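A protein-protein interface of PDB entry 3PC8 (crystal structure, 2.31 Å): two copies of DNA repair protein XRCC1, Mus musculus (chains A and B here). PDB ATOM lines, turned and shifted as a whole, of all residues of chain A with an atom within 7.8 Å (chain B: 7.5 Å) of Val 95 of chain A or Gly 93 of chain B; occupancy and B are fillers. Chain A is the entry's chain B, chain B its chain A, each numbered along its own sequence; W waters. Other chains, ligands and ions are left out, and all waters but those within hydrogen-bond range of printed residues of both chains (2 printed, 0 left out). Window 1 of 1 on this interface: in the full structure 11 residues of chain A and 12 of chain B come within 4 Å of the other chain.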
ATOM      1  N   GLN A  53     -17.156   1.306 -21.756  1.00  0.00           N
ATOM      2  CA  GLN A  53     -18.426   2.016 -21.745  1.00  0.00           C
ATOM      3  C   GLN A  53     -19.594   1.042 -21.581  1.00  0.00           C
ATOM      4  O   GLN A  53     -19.448  -0.160 -21.811  1.00  0.00           O
ATOM      5  CB  GLN A  53     -18.576   2.840 -23.028  1.00  0.00           C
ATOM      6  CG  GLN A  53     -17.386   3.762 -23.298  1.00  0.00           C
ATOM      7  CD  GLN A  53     -17.467   4.483 -24.638  1.00  0.00           C
ATOM      8  OE1 GLN A  53     -16.565   5.243 -25.001  1.00  0.00           O
ATOM      9  NE2 GLN A  53     -18.545   4.247 -25.379  1.00  0.00           N
ATOM     10  N   GLU A  54     -20.749   1.562 -21.176  1.00  0.00           N
ATOM     11  CA  GLU A  54     -21.944   0.736 -20.988  1.00  0.00           C
ATOM     12  C   GLU A  54     -22.343   0.059 -22.294  1.00  0.00           C
ATOM     13  O   GLU A  54     -21.883   0.453 -23.368  1.00  0.00           O
ATOM     14  CB  GLU A  54     -23.109   1.582 -20.462  1.00  0.00           C
ATOM     15  N   TRP A  55     -23.193  -0.960 -22.201  1.00  0.00           N
ATOM     16  CA  TRP A  55     -23.684  -1.637 -23.395  1.00  0.00           C
ATOM     17  C   TRP A  55     -24.112  -0.599 -24.418  1.00  0.00           C
ATOM     18  O   TRP A  55     -24.670   0.439 -24.065  1.00  0.00           O
ATOM     19  CB  TRP A  55     -24.858  -2.562 -23.062  1.00  0.00           C
ATOM     20  CG  TRP A  55     -25.365  -3.322 -24.253  1.00  0.00           C
ATOM     21  CD1 TRP A  55     -26.402  -2.974 -25.065  1.00  0.00           C
ATOM     22  CD2 TRP A  55     -24.845  -4.552 -24.772  1.00  0.00           C
ATOM     23  NE1 TRP A  55     -26.566  -3.913 -26.055  1.00  0.00           N
ATOM     24  CE2 TRP A  55     -25.620  -4.892 -25.898  1.00  0.00           C
ATOM     25  CE3 TRP A  55     -23.800  -5.401 -24.393  1.00  0.00           C
ATOM     26  CZ2 TRP A  55     -25.388  -6.044 -26.648  1.00  0.00           C
ATOM     27  CZ3 TRP A  55     -23.567  -6.542 -25.140  1.00  0.00           C
ATOM     28  CH2 TRP A  55     -24.361  -6.853 -26.255  1.00  0.00           C
ATOM     29  N   ASP A  56     -23.843  -0.872 -25.687  1.00  0.00           N
ATOM     30  CA  ASP A  56     -24.131   0.099 -26.730  1.00  0.00           C
ATOM     31  C   ASP A  56     -25.048  -0.476 -27.801  1.00  0.00           C
ATOM     32  O   ASP A  56     -24.874  -1.616 -28.224  1.00  0.00           O
ATOM     33  CB  ASP A  56     -22.826   0.577 -27.366  1.00  0.00           C
ATOM     34  CG  ASP A  56     -22.996   1.854 -28.146  1.00  0.00           C
ATOM     35  OD1 ASP A  56     -23.720   1.835 -29.162  1.00  0.00           O
ATOM     36  OD2 ASP A  56     -22.398   2.875 -27.748  1.00  0.00           O
ATOM     37  N   PHE A  59     -23.660  -2.246 -30.540  1.00  0.00           N
ATOM     38  CA  PHE A  59     -23.302  -3.641 -30.307  1.00  0.00           C
ATOM     39  C   PHE A  59     -24.310  -4.564 -30.974  1.00  0.00           C
ATOM     40  O   PHE A  59     -23.944  -5.557 -31.605  1.00  0.00           O
ATOM     41  CB  PHE A  59     -23.228  -3.952 -28.810  1.00  0.00           C
ATOM     42  CG  PHE A  59     -22.068  -3.300 -28.112  1.00  0.00           C
ATOM     43  CD1 PHE A  59     -21.126  -2.584 -28.832  1.00  0.00           C
ATOM     44  CD2 PHE A  59     -21.908  -3.417 -26.740  1.00  0.00           C
ATOM     45  CE1 PHE A  59     -20.052  -1.985 -28.193  1.00  0.00           C
ATOM     46  CE2 PHE A  59     -20.842  -2.819 -26.098  1.00  0.00           C
ATOM     47  CZ  PHE A  59     -19.912  -2.103 -26.823  1.00  0.00           C
ATOM     48  N   PHE A  71     -18.371  -9.424 -25.752  1.00  0.00           N
ATOM     49  CA  PHE A  71     -18.081  -8.078 -25.273  1.00  0.00           C
ATOM     50  C   PHE A  71     -17.471  -8.124 -23.875  1.00  0.00           C
ATOM     51  O   PHE A  71     -18.065  -8.679 -22.948  1.00  0.00           O
ATOM     52  CB  PHE A  71     -19.349  -7.221 -25.292  1.00  0.00           C
ATOM     53  CG  PHE A  71     -19.999  -7.137 -26.647  1.00  0.00           C
ATOM     54  CD1 PHE A  71     -20.892  -8.115 -27.064  1.00  0.00           C
ATOM     55  CD2 PHE A  71     -19.712  -6.089 -27.505  1.00  0.00           C
ATOM     56  CE1 PHE A  71     -21.491  -8.047 -28.311  1.00  0.00           C
ATOM     57  CE2 PHE A  71     -20.302  -6.017 -28.755  1.00  0.00           C
ATOM     58  CZ  PHE A  71     -21.195  -6.996 -29.161  1.00  0.00           C
ATOM     59  N   VAL A  72     -16.286  -7.540 -23.720  1.00  0.00           N
ATOM     60  CA  VAL A  72     -15.522  -7.730 -22.489  1.00  0.00           C
ATOM     61  C   VAL A  72     -14.946  -6.434 -21.922  1.00  0.00           C
ATOM     62  O   VAL A  72     -14.629  -5.503 -22.661  1.00  0.00           O
ATOM     63  CB  VAL A  72     -14.373  -8.749 -22.697  1.00  0.00           C
ATOM     64  CG1 VAL A  72     -13.926  -9.333 -21.356  1.00  0.00           C
ATOM     65  CG2 VAL A  72     -14.814  -9.861 -23.644  1.00  0.00           C
ATOM     66  N   ARG A  73     -14.822  -6.386 -20.600  1.00  0.00           N
ATOM     67  CA  ARG A  73     -14.185  -5.268 -19.918  1.00  0.00           C
ATOM     68  C   ARG A  73     -12.668  -5.357 -20.042  1.00  0.00           C
ATOM     69  O   ARG A  73     -12.111  -6.453 -20.167  1.00  0.00           O
ATOM     70  CB  ARG A  73     -14.569  -5.258 -18.438  1.00  0.00           C
ATOM     71  CG  ARG A  73     -16.035  -4.972 -18.170  1.00  0.00           C
ATOM     72  CD  ARG A  73     -16.465  -3.618 -18.717  1.00  0.00           C
ATOM     73  NE  ARG A  73     -17.866  -3.343 -18.405  1.00  0.00           N
ATOM     74  CZ  ARG A  73     -18.585  -2.378 -18.967  1.00  0.00           C
ATOM     75  NH1 ARG A  73     -18.038  -1.592 -19.884  1.00  0.00           N
ATOM     76  NH2 ARG A  73     -19.856  -2.205 -18.617  1.00  0.00           N
ATOM     77  N   GLN A  90     -15.663 -14.675 -19.889  1.00  0.00           N
ATOM     78  CA  GLN A  90     -17.020 -14.665 -19.351  1.00  0.00           C
ATOM     79  C   GLN A  90     -17.082 -14.034 -17.964  1.00  0.00           C
ATOM     80  O   GLN A  90     -18.110 -13.482 -17.581  1.00  0.00           O
ATOM     81  CB  GLN A  90     -17.622 -16.076 -19.327  1.00  0.00           C
ATOM     82  CG  GLN A  90     -17.821 -16.691 -20.707  1.00  0.00           C
ATOM     83  CD  GLN A  90     -16.661 -17.573 -21.129  1.00  0.00           C
ATOM     84  OE1 GLN A  90     -15.531 -17.410 -20.659  1.00  0.00           O
ATOM     85  NE2 GLN A  90     -16.938 -18.522 -22.017  1.00  0.00           N
ATOM     86  N   TYR A  92     -15.703 -11.450 -17.168  1.00  0.00           N
ATOM     87  CA  TYR A  92     -15.546 -10.007 -17.337  1.00  0.00           C
ATOM     88  C   TYR A  92     -16.479  -9.432 -18.405  1.00  0.00           C
ATOM     89  O   TYR A  92     -16.204  -8.377 -18.975  1.00  0.00           O
ATOM     90  CB  TYR A  92     -14.085  -9.684 -17.673  1.00  0.00           C
ATOM     91  CG  TYR A  92     -13.097 -10.343 -16.733  1.00  0.00           C
ATOM     92  CD1 TYR A  92     -12.759  -9.750 -15.525  1.00  0.00           C
ATOM     93  CD2 TYR A  92     -12.519 -11.563 -17.045  1.00  0.00           C
ATOM     94  CE1 TYR A  92     -11.864 -10.351 -14.655  1.00  0.00           C
ATOM     95  CE2 TYR A  92     -11.625 -12.171 -16.185  1.00  0.00           C
ATOM     96  CZ  TYR A  92     -11.300 -11.561 -14.990  1.00  0.00           C
ATOM     97  OH  TYR A  92     -10.410 -12.164 -14.123  1.00  0.00           O
ATOM     98  N   GLY A  93     -17.595 -10.118 -18.646  1.00  0.00           N
ATOM     99  CA  GLY A  93     -18.480  -9.791 -19.750  1.00  0.00           C
ATOM    100  C   GLY A  93     -19.280  -8.513 -19.587  1.00  0.00           C
ATOM    101  O   GLY A  93     -19.438  -7.998 -18.484  1.00  0.00           O
ATOM    102  N   VAL A  94     -19.777  -7.998 -20.707  1.00  0.00           N
ATOM    103  CA  VAL A  94     -20.619  -6.808 -20.712  1.00  0.00           C
ATOM    104  C   VAL A  94     -21.972  -7.154 -21.314  1.00  0.00           C
ATOM    105  O   VAL A  94     -22.045  -7.702 -22.412  1.00  0.00           O
ATOM    106  CB  VAL A  94     -19.999  -5.684 -21.546  1.00  0.00           C
ATOM    107  CG1 VAL A  94     -20.844  -4.424 -21.433  1.00  0.00           C
ATOM    108  CG2 VAL A  94     -18.569  -5.422 -21.102  1.00  0.00           C
ATOM    109  N   VAL A  95     -23.039  -6.830 -20.595  1.00  0.00           N
ATOM    110  CA  VAL A  95     -24.386  -7.164 -21.026  1.00  0.00           C
ATOM    111  C   VAL A  95     -25.301  -5.962 -20.855  1.00  0.00           C
ATOM    112  O   VAL A  95     -24.980  -5.039 -20.109  1.00  0.00           O
ATOM    113  CB  VAL A  95     -24.947  -8.347 -20.217  1.00  0.00           C
ATOM    114  CG1 VAL A  95     -24.075  -9.579 -20.411  1.00  0.00           C
ATOM    115  CG2 VAL A  95     -25.032  -7.979 -18.745  1.00  0.00           C
ATOM    116  N   PRO A  96     -26.446  -5.968 -21.552  1.00  0.00           N
ATOM    117  CA  PRO A  96     -27.403  -4.865 -21.435  1.00  0.00           C
ATOM    118  C   PRO A  96     -27.916  -4.721 -20.006  1.00  0.00           C
ATOM    119  O   PRO A  96     -27.924  -5.701 -19.255  1.00  0.00           O
ATOM    120  CB  PRO A  96     -28.542  -5.295 -22.363  1.00  0.00           C
ATOM    121  CG  PRO A  96     -27.900  -6.210 -23.350  1.00  0.00           C
ATOM    122  CD  PRO A  96     -26.862  -6.954 -22.564  1.00  0.00           C
ATOM    123  N   GLN A  97     -28.327  -3.510 -19.641  1.00  0.00           N
ATOM    124  CA  GLN A  97     -28.930  -3.257 -18.336  1.00  0.00           C
ATOM    125  C   GLN A  97     -30.120  -4.183 -18.108  1.00  0.00           C
ATOM    126  O   GLN A  97     -30.520  -4.428 -16.971  1.00  0.00           O
ATOM    127  CB  GLN A  97     -29.374  -1.795 -18.223  1.00  0.00           C
ATOM    128  N   TRP B  55     -24.866 -15.026 -10.721  1.00  0.00           N
ATOM    129  CA  TRP B  55     -23.631 -15.718 -11.074  1.00  0.00           C
ATOM    130  C   TRP B  55     -23.211 -16.686  -9.972  1.00  0.00           C
ATOM    131  O   TRP B  55     -23.389 -16.416  -8.784  1.00  0.00           O
ATOM    132  CB  TRP B  55     -22.504 -14.720 -11.347  1.00  0.00           C
ATOM    133  CG  TRP B  55     -21.218 -15.375 -11.765  1.00  0.00           C
ATOM    134  CD1 TRP B  55     -20.170 -15.717 -10.957  1.00  0.00           C
ATOM    135  CD2 TRP B  55     -20.848 -15.773 -13.091  1.00  0.00           C
ATOM    136  NE1 TRP B  55     -19.169 -16.291 -11.701  1.00  0.00           N
ATOM    137  CE2 TRP B  55     -19.563 -16.344 -13.012  1.00  0.00           C
ATOM    138  CE3 TRP B  55     -21.479 -15.698 -14.337  1.00  0.00           C
ATOM    139  CZ2 TRP B  55     -18.895 -16.835 -14.131  1.00  0.00           C
ATOM    140  CZ3 TRP B  55     -20.815 -16.185 -15.448  1.00  0.00           C
ATOM    141  CH2 TRP B  55     -19.533 -16.743 -15.338  1.00  0.00           C
ATOM    142  N   ALA B  70     -21.488 -20.371 -22.485  1.00  0.00           N
ATOM    143  CA  ALA B  70     -22.158 -19.083 -22.350  1.00  0.00           C
ATOM    144  C   ALA B  70     -23.255 -19.195 -21.296  1.00  0.00           C
ATOM    145  O   ALA B  70     -23.981 -20.186 -21.254  1.00  0.00           O
ATOM    146  CB  ALA B  70     -22.743 -18.649 -23.685  1.00  0.00           C
ATOM    147  N   PHE B  71     -23.374 -18.183 -20.445  1.00  0.00           N
ATOM    148  CA  PHE B  71     -24.388 -18.194 -19.398  1.00  0.00           C
ATOM    149  C   PHE B  71     -25.498 -17.198 -19.709  1.00  0.00           C
ATOM    150  O   PHE B  71     -25.244 -16.009 -19.876  1.00  0.00           O
ATOM    151  CB  PHE B  71     -23.744 -17.908 -18.039  1.00  0.00           C
ATOM    152  CG  PHE B  71     -22.663 -18.882 -17.680  1.00  0.00           C
ATOM    153  CD1 PHE B  71     -21.356 -18.671 -18.096  1.00  0.00           C
ATOM    154  CD2 PHE B  71     -22.954 -20.025 -16.951  1.00  0.00           C
ATOM    155  CE1 PHE B  71     -20.355 -19.574 -17.775  1.00  0.00           C
ATOM    156  CE2 PHE B  71     -21.958 -20.934 -16.626  1.00  0.00           C
ATOM    157  CZ  PHE B  71     -20.656 -20.708 -17.041  1.00  0.00           C
ATOM    158  N   VAL B  72     -26.733 -17.685 -19.786  1.00  0.00           N
ATOM    159  CA  VAL B  72     -27.823 -16.865 -20.311  1.00  0.00           C
ATOM    160  C   VAL B  72     -29.094 -16.893 -19.463  1.00  0.00           C
ATOM    161  O   VAL B  72     -29.378 -17.878 -18.771  1.00  0.00           O
ATOM    162  CB  VAL B  72     -28.196 -17.277 -21.754  1.00  0.00           C
ATOM    163  CG1 VAL B  72     -28.806 -16.103 -22.485  1.00  0.00           C
ATOM    164  CG2 VAL B  72     -26.973 -17.778 -22.501  1.00  0.00           C
ATOM    165  N   ARG B  73     -29.854 -15.804 -19.533  1.00  0.00           N
ATOM    166  CA  ARG B  73     -31.140 -15.706 -18.851  1.00  0.00           C
ATOM    167  C   ARG B  73     -32.211 -16.461 -19.633  1.00  0.00           C
ATOM    168  O   ARG B  73     -32.140 -16.553 -20.862  1.00  0.00           O
ATOM    169  CB  ARG B  73     -31.565 -14.241 -18.699  1.00  0.00           C
ATOM    170  CG  ARG B  73     -30.777 -13.447 -17.671  1.00  0.00           C
ATOM    171  CD  ARG B  73     -30.832 -14.128 -16.317  1.00  0.00           C
ATOM    172  NE  ARG B  73     -30.018 -13.449 -15.313  1.00  0.00           N
ATOM    173  CZ  ARG B  73     -29.590 -14.023 -14.191  1.00  0.00           C
ATOM    174  NH1 ARG B  73     -29.891 -15.293 -13.937  1.00  0.00           N
ATOM    175  NH2 ARG B  73     -28.851 -13.336 -13.327  1.00  0.00           N
ATOM    176  N   TRP B  76     -33.894 -14.966 -22.765  1.00  0.00           N
ATOM    177  CA  TRP B  76     -33.363 -15.208 -24.104  1.00  0.00           C
ATOM    178  C   TRP B  76     -34.244 -16.196 -24.873  1.00  0.00           C
ATOM    179  O   TRP B  76     -34.616 -15.962 -26.027  1.00  0.00           O
ATOM    180  CB  TRP B  76     -31.942 -15.762 -24.018  1.00  0.00           C
ATOM    181  CG  TRP B  76     -31.387 -16.187 -25.343  1.00  0.00           C
ATOM    182  CD1 TRP B  76     -31.534 -15.541 -26.541  1.00  0.00           C
ATOM    183  CD2 TRP B  76     -30.611 -17.363 -25.615  1.00  0.00           C
ATOM    184  NE1 TRP B  76     -30.891 -16.235 -27.537  1.00  0.00           N
ATOM    185  CE2 TRP B  76     -30.318 -17.358 -26.996  1.00  0.00           C
ATOM    186  CE3 TRP B  76     -30.135 -18.418 -24.823  1.00  0.00           C
ATOM    187  CZ2 TRP B  76     -29.564 -18.366 -27.605  1.00  0.00           C
ATOM    188  CZ3 TRP B  76     -29.387 -19.420 -25.430  1.00  0.00           C
ATOM    189  CH2 TRP B  76     -29.110 -19.388 -26.808  1.00  0.00           C
ATOM    190  N   PRO B  88     -29.577 -13.042 -30.540  1.00  0.00           N
ATOM    191  CA  PRO B  88     -28.244 -13.188 -29.936  1.00  0.00           C
ATOM    192  C   PRO B  88     -28.327 -13.387 -28.422  1.00  0.00           C
ATOM    193  O   PRO B  88     -28.972 -12.598 -27.733  1.00  0.00           O
ATOM    194  CB  PRO B  88     -27.555 -11.854 -30.260  1.00  0.00           C
ATOM    195  CG  PRO B  88     -28.372 -11.247 -31.396  1.00  0.00           C
ATOM    196  CD  PRO B  88     -29.778 -11.711 -31.135  1.00  0.00           C
ATOM    197  N   HIS B  89     -27.685 -14.436 -27.916  1.00  0.00           N
ATOM    198  CA  HIS B  89     -27.671 -14.705 -26.481  1.00  0.00           C
ATOM    199  C   HIS B  89     -26.937 -13.606 -25.706  1.00  0.00           C
ATOM    200  O   HIS B  89     -27.223 -13.378 -24.534  1.00  0.00           O
ATOM    201  CB  HIS B  89     -27.020 -16.058 -26.203  1.00  0.00           C
ATOM    202  CG  HIS B  89     -25.588 -16.136 -26.635  1.00  0.00           C
ATOM    203  ND1 HIS B  89     -24.543 -15.757 -25.820  1.00  0.00           N
ATOM    204  CD2 HIS B  89     -25.028 -16.534 -27.804  1.00  0.00           C
ATOM    205  CE1 HIS B  89     -23.401 -15.926 -26.464  1.00  0.00           C
ATOM    206  NE2 HIS B  89     -23.669 -16.392 -27.671  1.00  0.00           N
ATOM    207  N   GLN B  90     -26.002 -12.924 -26.366  1.00  0.00           N
ATOM    208  CA  GLN B  90     -25.205 -11.885 -25.713  1.00  0.00           C
ATOM    209  C   GLN B  90     -26.070 -10.791 -25.099  1.00  0.00           C
ATOM    210  O   GLN B  90     -25.660 -10.134 -24.138  1.00  0.00           O
ATOM    211  CB  GLN B  90     -24.203 -11.249 -26.686  1.00  0.00           C
ATOM    212  CG  GLN B  90     -23.121 -12.177 -27.215  1.00  0.00           C
ATOM    213  CD  GLN B  90     -23.509 -12.832 -28.524  1.00  0.00           C
ATOM    214  OE1 GLN B  90     -24.695 -13.008 -28.817  1.00  0.00           O
ATOM    215  NE2 GLN B  90     -22.511 -13.204 -29.318  1.00  0.00           N
ATOM    216  N   LEU B  91     -27.260 -10.590 -25.663  1.00  0.00           N
ATOM    217  CA  LEU B  91     -28.180  -9.577 -25.159  1.00  0.00           C
ATOM    218  C   LEU B  91     -28.756  -9.975 -23.801  1.00  0.00           C
ATOM    219  O   LEU B  91     -29.297  -9.134 -23.079  1.00  0.00           O
ATOM    220  CB  LEU B  91     -29.326  -9.346 -26.150  1.00  0.00           C
ATOM    221  CG  LEU B  91     -28.954  -8.835 -27.541  1.00  0.00           C
ATOM    222  CD1 LEU B  91     -30.187  -8.672 -28.411  1.00  0.00           C
ATOM    223  CD2 LEU B  91     -28.210  -7.523 -27.432  1.00  0.00           C
ATOM    224  N   TYR B  92     -28.634 -11.257 -23.456  1.00  0.00           N
ATOM    225  CA  TYR B  92     -29.284 -11.799 -22.269  1.00  0.00           C
ATOM    226  C   TYR B  92     -28.290 -12.478 -21.327  1.00  0.00           C
ATOM    227  O   TYR B  92     -28.663 -13.357 -20.552  1.00  0.00           O
ATOM    228  CB  TYR B  92     -30.371 -12.795 -22.688  1.00  0.00           C
ATOM    229  CG  TYR B  92     -31.367 -12.217 -23.671  1.00  0.00           C
ATOM    230  CD1 TYR B  92     -32.472 -11.495 -23.227  1.00  0.00           C
ATOM    231  CD2 TYR B  92     -31.189 -12.368 -25.041  1.00  0.00           C
ATOM    232  CE1 TYR B  92     -33.380 -10.951 -24.124  1.00  0.00           C
ATOM    233  CE2 TYR B  92     -32.095 -11.824 -25.951  1.00  0.00           C
ATOM    234  CZ  TYR B  92     -33.185 -11.120 -25.484  1.00  0.00           C
ATOM    235  OH  TYR B  92     -34.086 -10.584 -26.369  1.00  0.00           O
ATOM    236  N   GLY B  93     -27.030 -12.055 -21.390  1.00  0.00           N
ATOM    237  CA  GLY B  93     -25.954 -12.744 -20.700  1.00  0.00           C
ATOM    238  C   GLY B  93     -25.939 -12.612 -19.189  1.00  0.00           C
ATOM    239  O   GLY B  93     -26.525 -11.691 -18.618  1.00  0.00           O
ATOM    240  N   VAL B  94     -25.267 -13.552 -18.535  1.00  0.00           N
ATOM    241  CA  VAL B  94     -25.125 -13.515 -17.090  1.00  0.00           C
ATOM    242  C   VAL B  94     -23.647 -13.394 -16.719  1.00  0.00           C
ATOM    243  O   VAL B  94     -22.822 -14.194 -17.159  1.00  0.00           O
ATOM    244  CB  VAL B  94     -25.728 -14.767 -16.451  1.00  0.00           C
ATOM    245  CG1 VAL B  94     -25.731 -14.639 -14.937  1.00  0.00           C
ATOM    246  CG2 VAL B  94     -27.146 -14.989 -16.984  1.00  0.00           C
ATOM    247  N   VAL B  95     -23.320 -12.381 -15.921  1.00  0.00           N
ATOM    248  CA  VAL B  95     -21.943 -12.136 -15.507  1.00  0.00           C
ATOM    249  C   VAL B  95     -21.873 -11.943 -13.998  1.00  0.00           C
ATOM    250  O   VAL B  95     -22.886 -11.667 -13.360  1.00  0.00           O
ATOM    251  CB  VAL B  95     -21.370 -10.865 -16.170  1.00  0.00           C
ATOM    252  CG1 VAL B  95     -21.418 -10.975 -17.691  1.00  0.00           C
ATOM    253  CG2 VAL B  95     -22.121  -9.633 -15.682  1.00  0.00           C
HETATM  254  O   HOH W   1     -20.594 -14.430 -18.924  1.00  0.00           O
HETATM  255  O   HOH W   2     -22.809  -9.873 -23.939  1.00  0.00           O
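Water W2 lies within hydrogen-bond range of O of Val 94 of chain A (2.8 Å) and O of Gln 90 of chain B (2.9 Å). Water W1 bridges the backbone carbonyl oxygen of Val 94 of chain B (2.9 Å) and the backbone carbonyl oxygen of Gln 90 of chain A (3.0 Å).
Among the printed residues, pairs that only touch across the chains: Trp 55 of chain A with Leu 91 of chain B (3.3 Å), Gly 93 of chain A with Val 95 of chain B (3.7 Å), Val 95 of chain A with Gly 93 of chain B (3.7 Å), Pro 96 of chain A with Gln 90 of chain B (3.7 Å) and Pro 96 of chain A with Leu 91 of chain B (3.3 Å).
Gly 93 of chain A touches Val 95 of chain B, and with the chains exchanged Val 95 of chain A touches Gly 93 of chain B.
Of the printed residues of chain B, Pro 96 of chain A touches Gln 90 (3.7 Å) and Leu 91 (3.3 Å). Trp 76 of chain B touches none of the printed residues of chain A. Of the printed residues of chain A, Gln 90 of chain B touches Pro 96. Of the printed residues of chain A, Leu 91 of chain B touches Trp 55 and Pro 96. Of the printed residues of chain A, Gly 93 of chain B touches Val 95 (3.7 Å). Printed residues of chain A within 4 Å of Val 95 of chain B: Gly 93. The nearest residue of chain A that does not touch Gly 93 of chain B is Pro 96 of chain A (5.2 Å). The nearest printed residue of chain B that does not touch Pro 96 of chain A is Tyr 92 of chain B (4.7 Å).
Printed residues of chain A that touch a printed residue of chain B: Trp 55, Gly 93, Val 95 and Pro 96. Hydrophobic or aromatic side chains of chain A that line the printed part of chain B: Trp 55, Val 95 and Pro 96. Along chain A the printed residues that touch a printed residue of chain B span positions 55 to 96. Among the printed residues, 5 pairs touch across the chains.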
